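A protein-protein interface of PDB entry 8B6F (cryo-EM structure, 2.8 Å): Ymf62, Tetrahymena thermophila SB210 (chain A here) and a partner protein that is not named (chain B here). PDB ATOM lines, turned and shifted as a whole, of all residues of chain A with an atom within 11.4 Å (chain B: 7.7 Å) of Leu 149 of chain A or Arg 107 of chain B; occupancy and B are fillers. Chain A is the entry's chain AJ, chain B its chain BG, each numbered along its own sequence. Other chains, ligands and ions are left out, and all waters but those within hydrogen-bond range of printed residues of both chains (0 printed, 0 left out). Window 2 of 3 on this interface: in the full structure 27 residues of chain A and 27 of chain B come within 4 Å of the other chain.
NH2 of Arg 107 of chain B lies within hydrogen-bond range of OD1 of Asn 108 of chain B (3.2 Å).
The backbone carbonyl oxygen (O) of Leu 104 of chain B lies within hydrogen-bond range of the side-chain amide nitrogen (ND2) of Asn 108 of chain B, at 3.4 Å.
Leu 149 of chain A touches two residues of chain B.
Of chain A, only Glu 148 (2.8 Å) and Leu 149 (3.9 Å) come within 4 Å of Arg 107 of chain B.
Leu 104 of chain B touches one residue of chain A.
No residue of chain A comes within 4 Å of Glu 106 of chain B.
No residue of chain A comes within 4 Å of Asp 109 of chain B.
No residue of chain A comes within 4 Å of Met 110 of chain B.
No residue of chain A comes within 4 Å of Leu 111 of chain B.
Printed residues of chain B within 4 Å of Phe 151 of chain A: His 101, Leu 104, Arg 105 and Asn 108.
Printed residues of chain A within 4 Å of Arg 105 of chain B: Phe 151.
Of the printed residues of chain A, His 101 of chain B touches Phe 151 and Ile 152.
Of the printed residues of chain B, Ile 152 of chain A touches His 101.
Ser 150 of chain A touches none of the printed residues of chain B.
Pro 146 of chain A touches none of the printed residues of chain B.
The nearest residue of chain B that does not touch Leu 149 of chain A is Leu 111 of chain B (4.5 Å).
The nearest residue of chain A that does not touch Arg 107 of chain B is Ser 150 of chain A (5.7 Å).
Among the printed residues, merely in contact across the chains: Phe 151 of chain A with Asn 108 of chain B, Phe 151 of chain A with His 101 of chain B, Phe 151 of chain A with Arg 105 of chain B, Phe 151 of chain A with Leu 104 of chain B, Leu 149 of chain A with Arg 107 of chain B and Ile 152 of chain A with His 101 of chain B.
The backbone carbonyl oxygen (O) of Glu 148 of chain A sits at hydrogen-bond distance from the guanidinium group (NH2) of Arg 107 of chain B (2.8 Å).
The backbone carbonyl oxygen (O) of Leu 149 of chain A is in hydrogen-bond range of the side-chain amide nitrogen (ND2) of Asn 108 of chain B (3.1 Å).
Of the 15 printed residues of chain A, 4 touch a printed residue of chain B.
Along chain A the printed residues that touch a printed residue of chain B span positions 148 to 152.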
ATOM      1  N   GLU A 140      23.283  35.571   5.068  1.00  0.00           N
ATOM      2  CA  GLU A 140      22.995  36.382   6.240  1.00  0.00           C
ATOM      3  C   GLU A 140      24.006  37.513   6.359  1.00  0.00           C
ATOM      4  O   GLU A 140      25.206  37.310   6.157  1.00  0.00           O
ATOM      5  CB  GLU A 140      23.018  35.525   7.508  1.00  0.00           C
ATOM      6  CG  GLU A 140      24.398  35.018   7.882  1.00  0.00           C
ATOM      7  CD  GLU A 140      24.353  33.971   8.975  1.00  0.00           C
ATOM      8  OE1 GLU A 140      23.276  33.378   9.187  1.00  0.00           O
ATOM      9  OE2 GLU A 140      25.395  33.743   9.624  1.00  0.00           O
ATOM     10  N   LEU A 141      23.509  38.701   6.686  1.00  0.00           N
ATOM     11  CA  LEU A 141      24.375  39.853   6.880  1.00  0.00           C
ATOM     12  C   LEU A 141      25.255  39.670   8.109  1.00  0.00           C
ATOM     13  O   LEU A 141      24.923  38.928   9.035  1.00  0.00           O
ATOM     14  CB  LEU A 141      23.544  41.126   7.049  1.00  0.00           C
ATOM     15  CG  LEU A 141      22.976  41.779   5.793  1.00  0.00           C
ATOM     16  CD1 LEU A 141      21.949  42.831   6.168  1.00  0.00           C
ATOM     17  CD2 LEU A 141      24.090  42.394   4.969  1.00  0.00           C
ATOM     18  N   LEU A 143      26.481  41.039  11.598  1.00  0.00           N
ATOM     19  CA  LEU A 143      25.671  41.554  12.698  1.00  0.00           C
ATOM     20  C   LEU A 143      24.346  40.808  12.793  1.00  0.00           C
ATOM     21  O   LEU A 143      23.548  41.112  13.687  1.00  0.00           O
ATOM     22  CB  LEU A 143      25.379  43.060  12.586  1.00  0.00           C
ATOM     23  CG  LEU A 143      26.599  43.969  12.447  1.00  0.00           C
ATOM     24  CD1 LEU A 143      26.181  45.361  12.017  1.00  0.00           C
ATOM     25  CD2 LEU A 143      27.365  44.016  13.758  1.00  0.00           C
ATOM     26  N   PHE A 144      24.077  39.851  11.905  1.00  0.00           N
ATOM     27  CA  PHE A 144      22.880  39.031  12.046  1.00  0.00           C
ATOM     28  C   PHE A 144      22.906  38.262  13.358  1.00  0.00           C
ATOM     29  O   PHE A 144      21.892  38.176  14.059  1.00  0.00           O
ATOM     30  CB  PHE A 144      22.768  38.077  10.857  1.00  0.00           C
ATOM     31  CG  PHE A 144      21.593  37.148  10.930  1.00  0.00           C
ATOM     32  CD1 PHE A 144      20.343  37.557  10.503  1.00  0.00           C
ATOM     33  CD2 PHE A 144      21.744  35.859  11.412  1.00  0.00           C
ATOM     34  CE1 PHE A 144      19.263  36.701  10.564  1.00  0.00           C
ATOM     35  CE2 PHE A 144      20.670  34.999  11.474  1.00  0.00           C
ATOM     36  CZ  PHE A 144      19.427  35.419  11.049  1.00  0.00           C
ATOM     37  N   LEU A 145      24.056  37.705  13.709  1.00  0.00           N
ATOM     38  CA  LEU A 145      24.301  37.060  14.986  1.00  0.00           C
ATOM     39  C   LEU A 145      25.573  37.630  15.588  1.00  0.00           C
ATOM     40  O   LEU A 145      26.421  38.169  14.868  1.00  0.00           O
ATOM     41  CB  LEU A 145      24.438  35.537  14.839  1.00  0.00           C
ATOM     42  CG  LEU A 145      23.152  34.724  14.705  1.00  0.00           C
ATOM     43  CD1 LEU A 145      23.475  33.260  14.482  1.00  0.00           C
ATOM     44  CD2 LEU A 145      22.276  34.887  15.938  1.00  0.00           C
ATOM     45  N   PRO A 146      25.736  37.538  16.906  1.00  0.00           N
ATOM     46  CA  PRO A 146      26.965  38.047  17.523  1.00  0.00           C
ATOM     47  C   PRO A 146      28.193  37.359  16.950  1.00  0.00           C
ATOM     48  O   PRO A 146      28.181  36.161  16.658  1.00  0.00           O
ATOM     49  CB  PRO A 146      26.778  37.722  19.009  1.00  0.00           C
ATOM     50  CG  PRO A 146      25.310  37.595  19.191  1.00  0.00           C
ATOM     51  CD  PRO A 146      24.785  37.030  17.910  1.00  0.00           C
ATOM     52  N   LEU A 147      29.265  38.136  16.783  1.00  0.00           N
ATOM     53  CA  LEU A 147      30.510  37.576  16.275  1.00  0.00           C
ATOM     54  C   LEU A 147      31.091  36.532  17.215  1.00  0.00           C
ATOM     55  O   LEU A 147      31.892  35.699  16.781  1.00  0.00           O
ATOM     56  CB  LEU A 147      31.529  38.694  16.045  1.00  0.00           C
ATOM     57  CG  LEU A 147      32.915  38.258  15.563  1.00  0.00           C
ATOM     58  CD1 LEU A 147      32.829  37.577  14.207  1.00  0.00           C
ATOM     59  CD2 LEU A 147      33.852  39.447  15.507  1.00  0.00           C
ATOM     60  N   GLU A 148      30.708  36.558  18.492  1.00  0.00           N
ATOM     61  CA  GLU A 148      31.284  35.638  19.463  1.00  0.00           C
ATOM     62  C   GLU A 148      30.780  34.213  19.284  1.00  0.00           C
ATOM     63  O   GLU A 148      31.377  33.285  19.841  1.00  0.00           O
ATOM     64  CB  GLU A 148      30.985  36.128  20.879  1.00  0.00           C
ATOM     65  CG  GLU A 148      31.762  37.382  21.273  1.00  0.00           C
ATOM     66  CD  GLU A 148      31.272  38.626  20.564  1.00  0.00           C
ATOM     67  OE1 GLU A 148      30.368  38.510  19.712  1.00  0.00           O
ATOM     68  OE2 GLU A 148      31.786  39.723  20.865  1.00  0.00           O
ATOM     69  N   LEU A 149      29.698  34.017  18.531  1.00  0.00           N
ATOM     70  CA  LEU A 149      29.226  32.667  18.251  1.00  0.00           C
ATOM     71  C   LEU A 149      30.076  31.974  17.195  1.00  0.00           C
ATOM     72  O   LEU A 149      30.221  30.747  17.230  1.00  0.00           O
ATOM     73  CB  LEU A 149      27.763  32.701  17.805  1.00  0.00           C
ATOM     74  CG  LEU A 149      26.756  33.266  18.810  1.00  0.00           C
ATOM     75  CD1 LEU A 149      25.348  33.170  18.252  1.00  0.00           C
ATOM     76  CD2 LEU A 149      26.844  32.560  20.152  1.00  0.00           C
ATOM     77  N   SER A 150      30.639  32.729  16.255  1.00  0.00           N
ATOM     78  CA  SER A 150      31.500  32.154  15.232  1.00  0.00           C
ATOM     79  C   SER A 150      32.867  31.842  15.827  1.00  0.00           C
ATOM     80  O   SER A 150      33.457  32.675  16.520  1.00  0.00           O
ATOM     81  CB  SER A 150      31.639  33.118  14.055  1.00  0.00           C
ATOM     82  OG  SER A 150      32.459  32.568  13.039  1.00  0.00           O
ATOM     83  N   PHE A 151      33.371  30.637  15.552  1.00  0.00           N
ATOM     84  CA  PHE A 151      34.627  30.186  16.139  1.00  0.00           C
ATOM     85  C   PHE A 151      35.578  29.513  15.162  1.00  0.00           C
ATOM     86  O   PHE A 151      36.735  29.289  15.527  1.00  0.00           O
ATOM     87  CB  PHE A 151      34.345  29.210  17.289  1.00  0.00           C
ATOM     88  CG  PHE A 151      33.559  28.002  16.875  1.00  0.00           C
ATOM     89  CD1 PHE A 151      32.175  28.042  16.839  1.00  0.00           C
ATOM     90  CD2 PHE A 151      34.200  26.828  16.521  1.00  0.00           C
ATOM     91  CE1 PHE A 151      31.445  26.935  16.457  1.00  0.00           C
ATOM     92  CE2 PHE A 151      33.473  25.715  16.136  1.00  0.00           C
ATOM     93  CZ  PHE A 151      32.095  25.770  16.105  1.00  0.00           C
ATOM     94  N   ILE A 152      35.144  29.179  13.947  1.00  0.00           N
ATOM     95  CA  ILE A 152      35.977  28.372  13.062  1.00  0.00           C
ATOM     96  C   ILE A 152      37.217  29.142  12.624  1.00  0.00           C
ATOM     97  O   ILE A 152      38.293  28.559  12.450  1.00  0.00           O
ATOM     98  CB  ILE A 152      35.152  27.879  11.858  1.00  0.00           C
ATOM     99  CG1 ILE A 152      35.963  26.889  11.019  1.00  0.00           C
ATOM    100  CG2 ILE A 152      34.699  29.050  11.002  1.00  0.00           C
ATOM    101  CD1 ILE A 152      36.435  25.662  11.783  1.00  0.00           C
ATOM    102  N   ASP A 153      37.092  30.456  12.430  1.00  0.00           N
ATOM    103  CA  ASP A 153      38.220  31.242  11.944  1.00  0.00           C
ATOM    104  C   ASP A 153      39.423  31.167  12.875  1.00  0.00           C
ATOM    105  O   ASP A 153      40.550  31.409  12.431  1.00  0.00           O
ATOM    106  CB  ASP A 153      37.801  32.701  11.757  1.00  0.00           C
ATOM    107  CG  ASP A 153      36.768  32.875  10.662  1.00  0.00           C
ATOM    108  OD1 ASP A 153      36.754  32.054   9.721  1.00  0.00           O
ATOM    109  OD2 ASP A 153      35.967  33.828  10.743  1.00  0.00           O
ATOM    110  N   ILE A 154      39.213  30.843  14.151  1.00  0.00           N
ATOM    111  CA  ILE A 154      40.331  30.710  15.078  1.00  0.00           C
ATOM    112  C   ILE A 154      41.038  29.369  14.919  1.00  0.00           C
ATOM    113  O   ILE A 154      42.194  29.234  15.336  1.00  0.00           O
ATOM    114  CB  ILE A 154      39.857  30.893  16.533  1.00  0.00           C
ATOM    115  CG1 ILE A 154      39.299  32.303  16.765  1.00  0.00           C
ATOM    116  CG2 ILE A 154      40.988  30.639  17.525  1.00  0.00           C
ATOM    117  CD1 ILE A 154      37.875  32.527  16.277  1.00  0.00           C
ATOM    118  N   TYR A 155      40.386  28.379  14.314  1.00  0.00           N
ATOM    119  CA  TYR A 155      40.998  27.066  14.165  1.00  0.00           C
ATOM    120  C   TYR A 155      42.220  27.138  13.259  1.00  0.00           C
ATOM    121  O   TYR A 155      42.202  27.788  12.211  1.00  0.00           O
ATOM    122  CB  TYR A 155      39.982  26.074  13.598  1.00  0.00           C
ATOM    123  CG  TYR A 155      40.548  24.695  13.356  1.00  0.00           C
ATOM    124  CD1 TYR A 155      40.567  23.745  14.368  1.00  0.00           C
ATOM    125  CD2 TYR A 155      41.048  24.338  12.113  1.00  0.00           C
ATOM    126  CE1 TYR A 155      41.082  22.483  14.151  1.00  0.00           C
ATOM    127  CE2 TYR A 155      41.565  23.080  11.884  1.00  0.00           C
ATOM    128  CZ  TYR A 155      41.578  22.156  12.907  1.00  0.00           C
ATOM    129  OH  TYR A 155      42.091  20.900  12.682  1.00  0.00           O
ATOM    130  N   HIS B 101      39.167  25.016  20.574  1.00  0.00           N
ATOM    131  CA  HIS B 101      38.077  24.863  19.619  1.00  0.00           C
ATOM    132  C   HIS B 101      36.933  24.057  20.219  1.00  0.00           C
ATOM    133  O   HIS B 101      35.760  24.407  20.050  1.00  0.00           O
ATOM    134  CB  HIS B 101      38.604  24.195  18.350  1.00  0.00           C
ATOM    135  CG  HIS B 101      37.598  24.099  17.248  1.00  0.00           C
ATOM    136  ND1 HIS B 101      36.908  22.940  16.971  1.00  0.00           N
ATOM    137  CD2 HIS B 101      37.170  25.016  16.349  1.00  0.00           C
ATOM    138  CE1 HIS B 101      36.096  23.147  15.950  1.00  0.00           C
ATOM    139  NE2 HIS B 101      36.237  24.397  15.552  1.00  0.00           N
ATOM    140  N   LEU B 102      37.257  22.972  20.923  1.00  0.00           N
ATOM    141  CA  LEU B 102      36.225  22.145  21.542  1.00  0.00           C
ATOM    142  C   LEU B 102      35.537  22.863  22.695  1.00  0.00           C
ATOM    143  O   LEU B 102      34.340  22.652  22.925  1.00  0.00           O
ATOM    144  CB  LEU B 102      36.832  20.827  22.019  1.00  0.00           C
ATOM    145  CG  LEU B 102      37.356  19.917  20.906  1.00  0.00           C
ATOM    146  CD1 LEU B 102      38.088  18.727  21.493  1.00  0.00           C
ATOM    147  CD2 LEU B 102      36.224  19.449  20.005  1.00  0.00           C
ATOM    148  N   ALA B 103      36.262  23.706  23.431  1.00  0.00           N
ATOM    149  CA  ALA B 103      35.625  24.496  24.479  1.00  0.00           C
ATOM    150  C   ALA B 103      34.589  25.445  23.890  1.00  0.00           C
ATOM    151  O   ALA B 103      33.478  25.572  24.415  1.00  0.00           O
ATOM    152  CB  ALA B 103      36.679  25.271  25.268  1.00  0.00           C
ATOM    153  N   LEU B 104      34.942  26.135  22.804  1.00  0.00           N
ATOM    154  CA  LEU B 104      33.974  27.016  22.158  1.00  0.00           C
ATOM    155  C   LEU B 104      32.790  26.223  21.623  1.00  0.00           C
ATOM    156  O   LEU B 104      31.640  26.665  21.722  1.00  0.00           O
ATOM    157  CB  LEU B 104      34.642  27.808  21.036  1.00  0.00           C
ATOM    158  CG  LEU B 104      35.214  29.156  21.482  1.00  0.00           C
ATOM    159  CD1 LEU B 104      36.397  28.951  22.403  1.00  0.00           C
ATOM    160  CD2 LEU B 104      35.608  30.013  20.294  1.00  0.00           C
ATOM    161  N   ARG B 105      33.053  25.049  21.042  1.00  0.00           N
ATOM    162  CA  ARG B 105      31.969  24.210  20.543  1.00  0.00           C
ATOM    163  C   ARG B 105      31.049  23.761  21.669  1.00  0.00           C
ATOM    164  O   ARG B 105      29.824  23.728  21.504  1.00  0.00           O
ATOM    165  CB  ARG B 105      32.536  22.999  19.803  1.00  0.00           C
ATOM    166  CG  ARG B 105      32.903  23.289  18.357  1.00  0.00           C
ATOM    167  CD  ARG B 105      33.477  22.068  17.657  1.00  0.00           C
ATOM    168  NE  ARG B 105      32.575  20.924  17.702  1.00  0.00           N
ATOM    169  CZ  ARG B 105      32.817  19.757  17.121  1.00  0.00           C
ATOM    170  NH1 ARG B 105      33.926  19.543  16.433  1.00  0.00           N
ATOM    171  NH2 ARG B 105      31.920  18.780  17.231  1.00  0.00           N
ATOM    172  N   GLU B 106      31.617  23.411  22.826  1.00  0.00           N
ATOM    173  CA  GLU B 106      30.787  23.019  23.960  1.00  0.00           C
ATOM    174  C   GLU B 106      29.912  24.173  24.429  1.00  0.00           C
ATOM    175  O   GLU B 106      28.727  23.982  24.722  1.00  0.00           O
ATOM    176  CB  GLU B 106      31.660  22.516  25.108  1.00  0.00           C
ATOM    177  CG  GLU B 106      32.237  21.129  24.879  1.00  0.00           C
ATOM    178  CD  GLU B 106      33.035  20.631  26.064  1.00  0.00           C
ATOM    179  OE1 GLU B 106      33.290  21.434  26.986  1.00  0.00           O
ATOM    180  OE2 GLU B 106      33.403  19.438  26.078  1.00  0.00           O
ATOM    181  N   ARG B 107      30.475  25.379  24.509  1.00  0.00           N
ATOM    182  CA  ARG B 107      29.672  26.534  24.889  1.00  0.00           C
ATOM    183  C   ARG B 107      28.525  26.736  23.907  1.00  0.00           C
ATOM    184  O   ARG B 107      27.377  26.958  24.308  1.00  0.00           O
ATOM    185  CB  ARG B 107      30.548  27.783  24.962  1.00  0.00           C
ATOM    186  CG  ARG B 107      29.800  29.034  25.398  1.00  0.00           C
ATOM    187  CD  ARG B 107      30.652  30.279  25.245  1.00  0.00           C
ATOM    188  NE  ARG B 107      31.048  30.501  23.859  1.00  0.00           N
ATOM    189  CZ  ARG B 107      30.285  31.079  22.942  1.00  0.00           C
ATOM    190  NH1 ARG B 107      29.066  31.503  23.225  1.00  0.00           N
ATOM    191  NH2 ARG B 107      30.759  31.236  21.710  1.00  0.00           N
ATOM    192  N   ASN B 108      28.820  26.664  22.607  1.00  0.00           N
ATOM    193  CA  ASN B 108      27.781  26.859  21.602  1.00  0.00           C
ATOM    194  C   ASN B 108      26.728  25.763  21.682  1.00  0.00           C
ATOM    195  O   ASN B 108      25.532  26.028  21.518  1.00  0.00           O
ATOM    196  CB  ASN B 108      28.400  26.905  20.205  1.00  0.00           C
ATOM    197  CG  ASN B 108      29.017  28.249  19.887  1.00  0.00           C
ATOM    198  OD1 ASN B 108      28.550  29.286  20.353  1.00  0.00           O
ATOM    199  ND2 ASN B 108      30.073  28.239  19.086  1.00  0.00           N
ATOM    200  N   ASP B 109      27.150  24.522  21.929  1.00  0.00           N
ATOM    201  CA  ASP B 109      26.185  23.436  22.050  1.00  0.00           C
ATOM    202  C   ASP B 109      25.264  23.655  23.243  1.00  0.00           C
ATOM    203  O   ASP B 109      24.051  23.441  23.146  1.00  0.00           O
ATOM    204  CB  ASP B 109      26.913  22.097  22.174  1.00  0.00           C
ATOM    205  CG  ASP B 109      27.705  21.747  20.929  1.00  0.00           C
ATOM    206  OD1 ASP B 109      27.670  22.533  19.960  1.00  0.00           O
ATOM    207  OD2 ASP B 109      28.361  20.684  20.918  1.00  0.00           O
ATOM    208  N   MET B 110      25.819  24.079  24.379  1.00  0.00           N
ATOM    209  CA  MET B 110      24.986  24.360  25.543  1.00  0.00           C
ATOM    210  C   MET B 110      23.989  25.471  25.242  1.00  0.00           C
ATOM    211  O   MET B 110      22.806  25.368  25.580  1.00  0.00           O
ATOM    212  CB  MET B 110      25.864  24.740  26.734  1.00  0.00           C
ATOM    213  CG  MET B 110      26.624  23.575  27.339  1.00  0.00           C
ATOM    214  SD  MET B 110      27.877  24.102  28.524  1.00  0.00           S
ATOM    215  CE  MET B 110      26.900  25.097  29.646  1.00  0.00           C
ATOM    216  N   LEU B 111      24.455  26.549  24.609  1.00  0.00           N
ATOM    217  CA  LEU B 111      23.558  27.655  24.291  1.00  0.00           C
ATOM    218  C   LEU B 111      22.457  27.206  23.339  1.00  0.00           C
ATOM    219  O   LEU B 111      21.281  27.531  23.540  1.00  0.00           O
ATOM    220  CB  LEU B 111      24.352  28.818  23.696  1.00  0.00           C
ATOM    221  CG  LEU B 111      23.540  30.058  23.306  1.00  0.00           C
ATOM    222  CD1 LEU B 111      24.297  31.322  23.650  1.00  0.00           C
ATOM    223  CD2 LEU B 111      23.193  30.045  21.830  1.00  0.00           C
ATOM    224  N   TYR B 112      22.818  26.448  22.300  1.00  0.00           N
ATOM    225  CA  TYR B 112      21.820  25.983  21.342  1.00  0.00           C
ATOM    226  C   TYR B 112      20.799  25.071  22.009  1.00  0.00           C
ATOM    227  O   TYR B 112      19.594  25.195  21.767  1.00  0.00           O
ATOM    228  CB  TYR B 112      22.496  25.252  20.180  1.00  0.00           C
ATOM    229  CG  TYR B 112      23.360  26.119  19.287  1.00  0.00           C
ATOM    230  CD1 TYR B 112      23.474  27.487  19.498  1.00  0.00           C
ATOM    231  CD2 TYR B 112      24.054  25.562  18.221  1.00  0.00           C
ATOM    232  CE1 TYR B 112      24.257  28.274  18.677  1.00  0.00           C
ATOM    233  CE2 TYR B 112      24.840  26.341  17.394  1.00  0.00           C
ATOM    234  CZ  TYR B 112      24.938  27.697  17.627  1.00  0.00           C
ATOM    235  OH  TYR B 112      25.720  28.476  16.806  1.00  0.00           O
ATOM    236  N   ASN B 113      21.260  24.149  22.854  1.00  0.00           N
ATOM    237  CA  ASN B 113      20.331  23.257  23.539  1.00  0.00           C
ATOM    238  C   ASN B 113      19.370  24.039  24.424  1.00  0.00           C
ATOM    239  O   ASN B 113      18.164  23.773  24.426  1.00  0.00           O
ATOM    240  CB  ASN B 113      21.103  22.231  24.370  1.00  0.00           C
ATOM    241  CG  ASN B 113      21.854  21.234  23.512  1.00  0.00           C
ATOM    242  OD1 ASN B 113      21.426  20.903  22.406  1.00  0.00           O
ATOM    243  ND2 ASN B 113      22.980  20.745  24.019  1.00  0.00           N
ATOM    244  N   LEU B 115      18.417  27.157  24.114  1.00  0.00           N
ATOM    245  CA  LEU B 115      17.520  28.007  23.339  1.00  0.00           C
ATOM    246  C   LEU B 115      16.464  27.191  22.603  1.00  0.00           C
ATOM    247  O   LEU B 115      15.317  27.631  22.470  1.00  0.00           O
ATOM    248  CB  LEU B 115      18.321  28.855  22.351  1.00  0.00           C
ATOM    249  CG  LEU B 115      19.216  29.957  22.930  1.00  0.00           C
ATOM    250  CD1 LEU B 115      19.914  30.713  21.814  1.00  0.00           C
ATOM    251  CD2 LEU B 115      18.428  30.919  23.802  1.00  0.00           C
